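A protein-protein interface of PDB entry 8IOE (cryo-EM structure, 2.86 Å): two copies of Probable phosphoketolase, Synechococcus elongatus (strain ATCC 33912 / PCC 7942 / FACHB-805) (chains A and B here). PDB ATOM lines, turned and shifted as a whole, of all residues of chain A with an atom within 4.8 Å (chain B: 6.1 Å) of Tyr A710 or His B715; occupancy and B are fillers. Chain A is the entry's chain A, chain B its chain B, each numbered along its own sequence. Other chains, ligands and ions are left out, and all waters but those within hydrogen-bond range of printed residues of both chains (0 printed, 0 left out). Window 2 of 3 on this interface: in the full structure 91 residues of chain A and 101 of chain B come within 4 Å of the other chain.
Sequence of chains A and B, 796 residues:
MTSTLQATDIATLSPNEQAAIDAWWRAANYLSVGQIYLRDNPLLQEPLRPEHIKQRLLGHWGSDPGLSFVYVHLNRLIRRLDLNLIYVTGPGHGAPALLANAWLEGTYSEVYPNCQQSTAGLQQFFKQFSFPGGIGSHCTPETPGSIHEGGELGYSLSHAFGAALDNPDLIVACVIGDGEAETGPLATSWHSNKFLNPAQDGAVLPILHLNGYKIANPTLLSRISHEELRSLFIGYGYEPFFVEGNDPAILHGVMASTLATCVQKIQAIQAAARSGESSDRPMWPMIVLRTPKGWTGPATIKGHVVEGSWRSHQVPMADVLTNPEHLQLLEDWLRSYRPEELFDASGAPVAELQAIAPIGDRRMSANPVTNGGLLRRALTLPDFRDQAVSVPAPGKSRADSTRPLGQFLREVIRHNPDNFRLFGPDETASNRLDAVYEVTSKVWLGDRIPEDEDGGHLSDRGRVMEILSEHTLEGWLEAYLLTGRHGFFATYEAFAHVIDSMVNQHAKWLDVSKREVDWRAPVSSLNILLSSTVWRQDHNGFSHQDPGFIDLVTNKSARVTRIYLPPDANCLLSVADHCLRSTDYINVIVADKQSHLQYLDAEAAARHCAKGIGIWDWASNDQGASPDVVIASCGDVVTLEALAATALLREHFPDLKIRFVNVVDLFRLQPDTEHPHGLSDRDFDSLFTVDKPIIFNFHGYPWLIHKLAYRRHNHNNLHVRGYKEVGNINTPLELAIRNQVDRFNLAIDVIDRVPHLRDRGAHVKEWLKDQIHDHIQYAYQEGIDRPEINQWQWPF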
ATOM      1  N   HIS A 706      30.031   0.200   7.216  1.00  0.00           N
ATOM      2  CA  HIS A 706      29.879   1.455   7.940  1.00  0.00           C
ATOM      3  C   HIS A 706      30.189   1.296   9.421  1.00  0.00           C
ATOM      4  O   HIS A 706      30.644   2.251  10.059  1.00  0.00           O
ATOM      5  CB  HIS A 706      28.470   2.003   7.761  1.00  0.00           C
ATOM      6  CG  HIS A 706      28.207   2.555   6.398  1.00  0.00           C
ATOM      7  ND1 HIS A 706      28.691   3.776   5.986  1.00  0.00           N
ATOM      8  CD2 HIS A 706      27.500   2.059   5.356  1.00  0.00           C
ATOM      9  CE1 HIS A 706      28.300   4.007   4.747  1.00  0.00           C
ATOM     10  NE2 HIS A 706      27.575   2.980   4.342  1.00  0.00           N
ATOM     11  N   LYS A 707      29.937   0.116   9.989  1.00  0.00           N
ATOM     12  CA  LYS A 707      30.273  -0.111  11.389  1.00  0.00           C
ATOM     13  C   LYS A 707      31.776  -0.040  11.606  1.00  0.00           C
ATOM     14  O   LYS A 707      32.251   0.590  12.557  1.00  0.00           O
ATOM     15  CB  LYS A 707      29.745  -1.466  11.851  1.00  0.00           C
ATOM     16  CG  LYS A 707      30.047  -1.760  13.307  1.00  0.00           C
ATOM     17  CD  LYS A 707      29.961  -3.240  13.605  1.00  0.00           C
ATOM     18  CE  LYS A 707      28.607  -3.798  13.228  1.00  0.00           C
ATOM     19  NZ  LYS A 707      28.535  -5.269  13.439  1.00  0.00           N
ATOM     20  N   LEU A 708      32.541  -0.683  10.725  1.00  0.00           N
ATOM     21  CA  LEU A 708      33.987  -0.729  10.891  1.00  0.00           C
ATOM     22  C   LEU A 708      34.615   0.631  10.622  1.00  0.00           C
ATOM     23  O   LEU A 708      35.439   1.113  11.407  1.00  0.00           O
ATOM     24  CB  LEU A 708      34.577  -1.788   9.965  1.00  0.00           C
ATOM     25  CG  LEU A 708      33.929  -3.163  10.077  1.00  0.00           C
ATOM     26  CD1 LEU A 708      34.575  -4.133   9.116  1.00  0.00           C
ATOM     27  CD2 LEU A 708      34.029  -3.676  11.494  1.00  0.00           C
ATOM     28  N   ALA A 709      34.227   1.275   9.526  1.00  0.00           N
ATOM     29  CA  ALA A 709      34.846   2.519   9.091  1.00  0.00           C
ATOM     30  C   ALA A 709      34.083   3.747   9.564  1.00  0.00           C
ATOM     31  O   ALA A 709      34.063   4.767   8.870  1.00  0.00           O
ATOM     32  CB  ALA A 709      34.979   2.535   7.570  1.00  0.00           C
ATOM     33  N   TYR A 710      33.447   3.673  10.733  1.00  0.00           N
ATOM     34  CA  TYR A 710      32.664   4.810  11.204  1.00  0.00           C
ATOM     35  C   TYR A 710      33.557   5.942  11.693  1.00  0.00           C
ATOM     36  O   TYR A 710      33.287   7.115  11.413  1.00  0.00           O
ATOM     37  CB  TYR A 710      31.713   4.376  12.312  1.00  0.00           C
ATOM     38  CG  TYR A 710      30.844   5.498  12.819  1.00  0.00           C
ATOM     39  CD1 TYR A 710      30.004   6.191  11.959  1.00  0.00           C
ATOM     40  CD2 TYR A 710      30.846   5.854  14.158  1.00  0.00           C
ATOM     41  CE1 TYR A 710      29.202   7.212  12.416  1.00  0.00           C
ATOM     42  CE2 TYR A 710      30.045   6.874  14.624  1.00  0.00           C
ATOM     43  CZ  TYR A 710      29.227   7.549  13.749  1.00  0.00           C
ATOM     44  OH  TYR A 710      28.428   8.568  14.209  1.00  0.00           O
ATOM     45  N   ARG A 711      34.621   5.614  12.421  1.00  0.00           N
ATOM     46  CA  ARG A 711      35.478   6.635  13.006  1.00  0.00           C
ATOM     47  C   ARG A 711      36.419   7.275  11.997  1.00  0.00           C
ATOM     48  O   ARG A 711      37.110   8.237  12.347  1.00  0.00           O
ATOM     49  CB  ARG A 711      36.291   6.039  14.154  1.00  0.00           C
ATOM     50  CG  ARG A 711      35.451   5.351  15.210  1.00  0.00           C
ATOM     51  CD  ARG A 711      34.459   6.313  15.833  1.00  0.00           C
ATOM     52  NE  ARG A 711      33.595   5.649  16.802  1.00  0.00           N
ATOM     53  CZ  ARG A 711      32.617   6.248  17.467  1.00  0.00           C
ATOM     54  NH1 ARG A 711      32.350   7.532  17.295  1.00  0.00           N
ATOM     55  NH2 ARG A 711      31.888   5.541  18.325  1.00  0.00           N
ATOM     56  N   ARG A 712      36.472   6.767  10.771  1.00  0.00           N
ATOM     57  CA  ARG A 712      37.358   7.320   9.761  1.00  0.00           C
ATOM     58  C   ARG A 712      36.929   8.728   9.374  1.00  0.00           C
ATOM     59  O   ARG A 712      35.758   9.097   9.479  1.00  0.00           O
ATOM     60  CB  ARG A 712      37.374   6.428   8.525  1.00  0.00           C
ATOM     61  CG  ARG A 712      37.791   5.004   8.801  1.00  0.00           C
ATOM     62  CD  ARG A 712      39.202   4.950   9.334  1.00  0.00           C
ATOM     63  NE  ARG A 712      39.711   3.586   9.366  1.00  0.00           N
ATOM     64  CZ  ARG A 712      40.957   3.265   9.680  1.00  0.00           C
ATOM     65  NH1 ARG A 712      41.848   4.187   9.997  1.00  0.00           N
ATOM     66  NH2 ARG A 712      41.317   1.986   9.675  1.00  0.00           N
ATOM     67  N   HIS A 715      34.474   8.788   6.235  1.00  0.00           N
ATOM     68  CA  HIS A 715      33.337   7.879   6.311  1.00  0.00           C
ATOM     69  C   HIS A 715      32.128   8.430   5.570  1.00  0.00           C
ATOM     70  O   HIS A 715      31.351   7.666   4.987  1.00  0.00           O
ATOM     71  CB  HIS A 715      32.975   7.599   7.765  1.00  0.00           C
ATOM     72  CG  HIS A 715      31.653   6.921   7.928  1.00  0.00           C
ATOM     73  ND1 HIS A 715      30.572   7.534   8.520  1.00  0.00           N
ATOM     74  CD2 HIS A 715      31.231   5.693   7.552  1.00  0.00           C
ATOM     75  CE1 HIS A 715      29.542   6.707   8.513  1.00  0.00           C
ATOM     76  NE2 HIS A 715      29.917   5.581   7.932  1.00  0.00           N
ATOM     77  N   TRP B 703      25.714  -0.023  18.469  1.00  0.00           N
ATOM     78  CA  TRP B 703      25.748   0.340  17.063  1.00  0.00           C
ATOM     79  C   TRP B 703      24.409   0.148  16.366  1.00  0.00           C
ATOM     80  O   TRP B 703      24.200   0.705  15.283  1.00  0.00           O
ATOM     81  CB  TRP B 703      26.826  -0.470  16.351  1.00  0.00           C
ATOM     82  CG  TRP B 703      27.029   0.005  14.983  1.00  0.00           C
ATOM     83  CD1 TRP B 703      26.748  -0.665  13.837  1.00  0.00           C
ATOM     84  CD2 TRP B 703      27.503   1.295  14.593  1.00  0.00           C
ATOM     85  NE1 TRP B 703      27.050   0.115  12.754  1.00  0.00           N
ATOM     86  CE2 TRP B 703      27.508   1.328  13.190  1.00  0.00           C
ATOM     87  CE3 TRP B 703      27.941   2.421  15.295  1.00  0.00           C
ATOM     88  CZ2 TRP B 703      27.929   2.435  12.474  1.00  0.00           C
ATOM     89  CZ3 TRP B 703      28.355   3.519  14.583  1.00  0.00           C
ATOM     90  CH2 TRP B 703      28.342   3.520  13.187  1.00  0.00           C
ATOM     91  N   ILE B 705      21.589   1.363  17.136  1.00  0.00           N
ATOM     92  CA  ILE B 705      20.921   2.655  17.053  1.00  0.00           C
ATOM     93  C   ILE B 705      21.465   3.467  15.887  1.00  0.00           C
ATOM     94  O   ILE B 705      20.720   4.189  15.216  1.00  0.00           O
ATOM     95  CB  ILE B 705      21.062   3.406  18.385  1.00  0.00           C
ATOM     96  CG1 ILE B 705      20.542   2.540  19.525  1.00  0.00           C
ATOM     97  CG2 ILE B 705      20.306   4.712  18.341  1.00  0.00           C
ATOM     98  CD1 ILE B 705      19.122   2.090  19.333  1.00  0.00           C
ATOM     99  N   HIS B 706      22.767   3.363  15.623  1.00  0.00           N
ATOM    100  CA  HIS B 706      23.341   4.103  14.505  1.00  0.00           C
ATOM    101  C   HIS B 706      22.882   3.551  13.164  1.00  0.00           C
ATOM    102  O   HIS B 706      22.796   4.301  12.188  1.00  0.00           O
ATOM    103  CB  HIS B 706      24.861   4.085  14.585  1.00  0.00           C
ATOM    104  CG  HIS B 706      25.419   4.969  15.652  1.00  0.00           C
ATOM    105  ND1 HIS B 706      25.517   6.335  15.507  1.00  0.00           N
ATOM    106  CD2 HIS B 706      25.917   4.683  16.876  1.00  0.00           C
ATOM    107  CE1 HIS B 706      26.047   6.854  16.598  1.00  0.00           C
ATOM    108  NE2 HIS B 706      26.299   5.873  17.445  1.00  0.00           N
ATOM    109  N   LYS B 707      22.601   2.250  13.087  1.00  0.00           N
ATOM    110  CA  LYS B 707      22.088   1.683  11.845  1.00  0.00           C
ATOM    111  C   LYS B 707      20.716   2.247  11.514  1.00  0.00           C
ATOM    112  O   LYS B 707      20.442   2.614  10.367  1.00  0.00           O
ATOM    113  CB  LYS B 707      22.018   0.163  11.941  1.00  0.00           C
ATOM    114  CG  LYS B 707      21.558  -0.496  10.656  1.00  0.00           C
ATOM    115  CD  LYS B 707      21.002  -1.881  10.908  1.00  0.00           C
ATOM    116  CE  LYS B 707      22.008  -2.754  11.624  1.00  0.00           C
ATOM    117  NZ  LYS B 707      21.449  -4.094  11.944  1.00  0.00           N
ATOM    118  N   ALA B 709      19.154   5.075  12.759  1.00  0.00           N
ATOM    119  CA  ALA B 709      19.114   6.525  12.639  1.00  0.00           C
ATOM    120  C   ALA B 709      20.267   7.073  11.810  1.00  0.00           C
ATOM    121  O   ALA B 709      20.742   8.182  12.070  1.00  0.00           O
ATOM    122  CB  ALA B 709      19.110   7.167  14.024  1.00  0.00           C
ATOM    123  N   TYR B 710      20.733   6.316  10.817  1.00  0.00           N
ATOM    124  CA  TYR B 710      21.868   6.778  10.025  1.00  0.00           C
ATOM    125  C   TYR B 710      21.472   7.908   9.087  1.00  0.00           C
ATOM    126  O   TYR B 710      22.222   8.878   8.923  1.00  0.00           O
ATOM    127  CB  TYR B 710      22.471   5.619   9.236  1.00  0.00           C
ATOM    128  CG  TYR B 710      23.700   6.009   8.457  1.00  0.00           C
ATOM    129  CD1 TYR B 710      24.808   6.545   9.097  1.00  0.00           C
ATOM    130  CD2 TYR B 710      23.758   5.841   7.082  1.00  0.00           C
ATOM    131  CE1 TYR B 710      25.934   6.902   8.393  1.00  0.00           C
ATOM    132  CE2 TYR B 710      24.881   6.196   6.369  1.00  0.00           C
ATOM    133  CZ  TYR B 710      25.966   6.726   7.030  1.00  0.00           C
ATOM    134  OH  TYR B 710      27.089   7.082   6.323  1.00  0.00           O
ATOM    135  N   ARG B 711      20.298   7.809   8.466  1.00  0.00           N
ATOM    136  CA  ARG B 711      19.874   8.795   7.483  1.00  0.00           C
ATOM    137  C   ARG B 711      19.337  10.074   8.107  1.00  0.00           C
ATOM    138  O   ARG B 711      19.050  11.025   7.373  1.00  0.00           O
ATOM    139  CB  ARG B 711      18.811   8.193   6.565  1.00  0.00           C
ATOM    140  CG  ARG B 711      19.234   6.902   5.897  1.00  0.00           C
ATOM    141  CD  ARG B 711      20.467   7.112   5.041  1.00  0.00           C
ATOM    142  NE  ARG B 711      20.921   5.869   4.428  1.00  0.00           N
ATOM    143  CZ  ARG B 711      21.994   5.763   3.657  1.00  0.00           C
ATOM    144  NH1 ARG B 711      22.752   6.812   3.380  1.00  0.00           N
ATOM    145  NH2 ARG B 711      22.317   4.576   3.154  1.00  0.00           N
ATOM    146  N   ARG B 712      19.185  10.119   9.427  1.00  0.00           N
ATOM    147  CA  ARG B 712      18.659  11.305  10.084  1.00  0.00           C
ATOM    148  C   ARG B 712      19.632  12.470   9.963  1.00  0.00           C
ATOM    149  O   ARG B 712      20.843  12.287   9.825  1.00  0.00           O
ATOM    150  CB  ARG B 712      18.381  11.017  11.554  1.00  0.00           C
ATOM    151  CG  ARG B 712      17.403   9.890  11.786  1.00  0.00           C
ATOM    152  CD  ARG B 712      16.050  10.223  11.206  1.00  0.00           C
ATOM    153  NE  ARG B 712      15.038   9.267  11.631  1.00  0.00           N
ATOM    154  CZ  ARG B 712      13.748   9.376  11.354  1.00  0.00           C
ATOM    155  NH1 ARG B 712      13.278  10.389  10.646  1.00  0.00           N
ATOM    156  NH2 ARG B 712      12.909   8.447  11.797  1.00  0.00           N
ATOM    157  N   HIS B 713      19.081  13.683   9.999  1.00  0.00           N
ATOM    158  CA  HIS B 713      19.915  14.878   9.930  1.00  0.00           C
ATOM    159  C   HIS B 713      20.815  14.998  11.152  1.00  0.00           C
ATOM    160  O   HIS B 713      21.993  15.351  11.029  1.00  0.00           O
ATOM    161  CB  HIS B 713      19.041  16.122   9.789  1.00  0.00           C
ATOM    162  CG  HIS B 713      18.292  16.191   8.496  1.00  0.00           C
ATOM    163  ND1 HIS B 713      17.232  15.360   8.203  1.00  0.00           N
ATOM    164  CD2 HIS B 713      18.455  16.989   7.415  1.00  0.00           C
ATOM    165  CE1 HIS B 713      16.773  15.645   6.998  1.00  0.00           C
ATOM    166  NE2 HIS B 713      17.496  16.631   6.499  1.00  0.00           N
ATOM    167  N   ASN B 714      20.283  14.702  12.336  1.00  0.00           N
ATOM    168  CA  ASN B 714      21.020  14.859  13.583  1.00  0.00           C
ATOM    169  C   ASN B 714      21.745  13.588  14.000  1.00  0.00           C
ATOM    170  O   ASN B 714      21.963  13.369  15.198  1.00  0.00           O
ATOM    171  CB  ASN B 714      20.076  15.322  14.694  1.00  0.00           C
ATOM    172  CG  ASN B 714      20.790  16.113  15.772  1.00  0.00           C
ATOM    173  OD1 ASN B 714      21.829  16.721  15.523  1.00  0.00           O
ATOM    174  ND2 ASN B 714      20.238  16.106  16.977  1.00  0.00           N
ATOM    175  N   HIS B 715      22.119  12.735  13.045  1.00  0.00           N
ATOM    176  CA  HIS B 715      22.800  11.493  13.395  1.00  0.00           C
ATOM    177  C   HIS B 715      24.180  11.755  13.979  1.00  0.00           C
ATOM    178  O   HIS B 715      24.624  11.034  14.879  1.00  0.00           O
ATOM    179  CB  HIS B 715      22.912  10.587  12.175  1.00  0.00           C
ATOM    180  CG  HIS B 715      23.873   9.458  12.362  1.00  0.00           C
ATOM    181  ND1 HIS B 715      25.068   9.379  11.683  1.00  0.00           N
ATOM    182  CD2 HIS B 715      23.827   8.375  13.172  1.00  0.00           C
ATOM    183  CE1 HIS B 715      25.712   8.289  12.057  1.00  0.00           C
ATOM    184  NE2 HIS B 715      24.979   7.661  12.958  1.00  0.00           N
ATOM    185  N   ASN B 716      24.880  12.773  13.476  1.00  0.00           N
ATOM    186  CA  ASN B 716      26.223  13.065  13.960  1.00  0.00           C
ATOM    187  C   ASN B 716      26.237  13.517  15.412  1.00  0.00           C
ATOM    188  O   ASN B 716      27.283  13.433  16.062  1.00  0.00           O
ATOM    189  CB  ASN B 716      26.879  14.128  13.079  1.00  0.00           C
ATOM    190  CG  ASN B 716      25.988  15.327  12.855  1.00  0.00           C
ATOM    191  OD1 ASN B 716      24.911  15.434  13.439  1.00  0.00           O
ATOM    192  ND2 ASN B 716      26.433  16.243  12.004  1.00  0.00           N
ATOM    193  N   ASN B 717      25.112  13.998  15.934  1.00  0.00           N
ATOM    194  CA  ASN B 717      25.015  14.402  17.326  1.00  0.00           C
ATOM    195  C   ASN B 717      24.458  13.303  18.217  1.00  0.00           C
ATOM    196  O   ASN B 717      24.176  13.558  19.390  1.00  0.00           O
ATOM    197  CB  ASN B 717      24.152  15.656  17.452  1.00  0.00           C
ATOM    198  CG  ASN B 717      24.913  16.824  18.027  1.00  0.00           C
ATOM    199  OD1 ASN B 717      25.818  16.647  18.841  1.00  0.00           O
ATOM    200  ND2 ASN B 717      24.556  18.030  17.604  1.00  0.00           N
ATOM    201  N   LEU B 718      24.296  12.095  17.692  1.00  0.00           N
ATOM    202  CA  LEU B 718      23.737  10.988  18.450  1.00  0.00           C
ATOM    203  C   LEU B 718      24.861  10.191  19.092  1.00  0.00           C
ATOM    204  O   LEU B 718      25.769   9.719  18.402  1.00  0.00           O
ATOM    205  CB  LEU B 718      22.908  10.088  17.537  1.00  0.00           C
ATOM    206  CG  LEU B 718      21.596   9.506  18.054  1.00  0.00           C
ATOM    207  CD1 LEU B 718      20.809   8.930  16.898  1.00  0.00           C
ATOM    208  CD2 LEU B 718      21.840   8.445  19.098  1.00  0.00           C
ATOM    209  N   HIS B 719      24.798  10.044  20.410  1.00  0.00           N
ATOM    210  CA  HIS B 719      25.775   9.273  21.163  1.00  0.00           C
ATOM    211  C   HIS B 719      25.062   8.130  21.863  1.00  0.00           C
ATOM    212  O   HIS B 719      24.105   8.353  22.609  1.00  0.00           O
ATOM    213  CB  HIS B 719      26.502  10.152  22.177  1.00  0.00           C
ATOM    214  CG  HIS B 719      27.045  11.415  21.589  1.00  0.00           C
ATOM    215  ND1 HIS B 719      28.245  11.467  20.916  1.00  0.00           N
ATOM    216  CD2 HIS B 719      26.544  12.672  21.563  1.00  0.00           C
ATOM    217  CE1 HIS B 719      28.464  12.703  20.505  1.00  0.00           C
ATOM    218  NE2 HIS B 719      27.447  13.454  20.886  1.00  0.00           N
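Of the 8 printed residues of chain A, 4 touch a printed residue of chain B.
Hydrophobic or aromatic side chains of chain A that line the printed part of chain B: His A706, Tyr A710 and His A715.
Hydrophobic or aromatic side chains of chain B that line the printed part of chain A: Trp B703, His B706, Tyr B710 and His B715.
Among the printed residues, 7 pairs touch across the chains.
Among the printed residues, no Asp or Glu carboxylate lies within 4 Å of a Lys or Arg side-chain nitrogen of the other chain.
Printed residues of chain B within 4 Å of Tyr A710: Trp B703, His B706 and His B715.
Printed residues of chain A within 4 Å of His B715: Tyr A710 (3.5 Å).
Of the printed residues of chain A, His B706 touches Tyr A710.
Of the printed residues of chain A, Tyr B710 touches His A706 and His A715.
Ala B709 touches none of the printed residues of chain A.
Lys B707 touches none of the printed residues of chain A.
The nearest printed residue of chain B that does not touch Tyr A710 is Asn B716 (5.0 Å).
The nearest printed residue of chain A that does not touch Tyr B710 is Tyr A710 (5.2 Å).
Among the printed residues, pairs that only touch across the chains: Tyr A710 with Trp B703, Lys A707 with Trp B703, His A715 with Tyr B710, Tyr A710 with His B715, His A706 with Trp B703, His A706 with Tyr B710 and Tyr A710 with His B706.
His A706 touches Tyr B710, and with the chains exchanged Tyr A710 touches His B706.
Tyr A710 touches His B715, and with the chains exchanged His A715 touches Tyr B710.
7 positions are printed for both chains.
A ring nitrogen (NE2) of His A715 sits at hydrogen-bond distance from a ring nitrogen (ND1) of His A706 (2.9 Å).
A ring nitrogen (ND1) of His B706 lies within hydrogen-bond range of a ring nitrogen (NE2) of His B715, 2.9 Å away.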
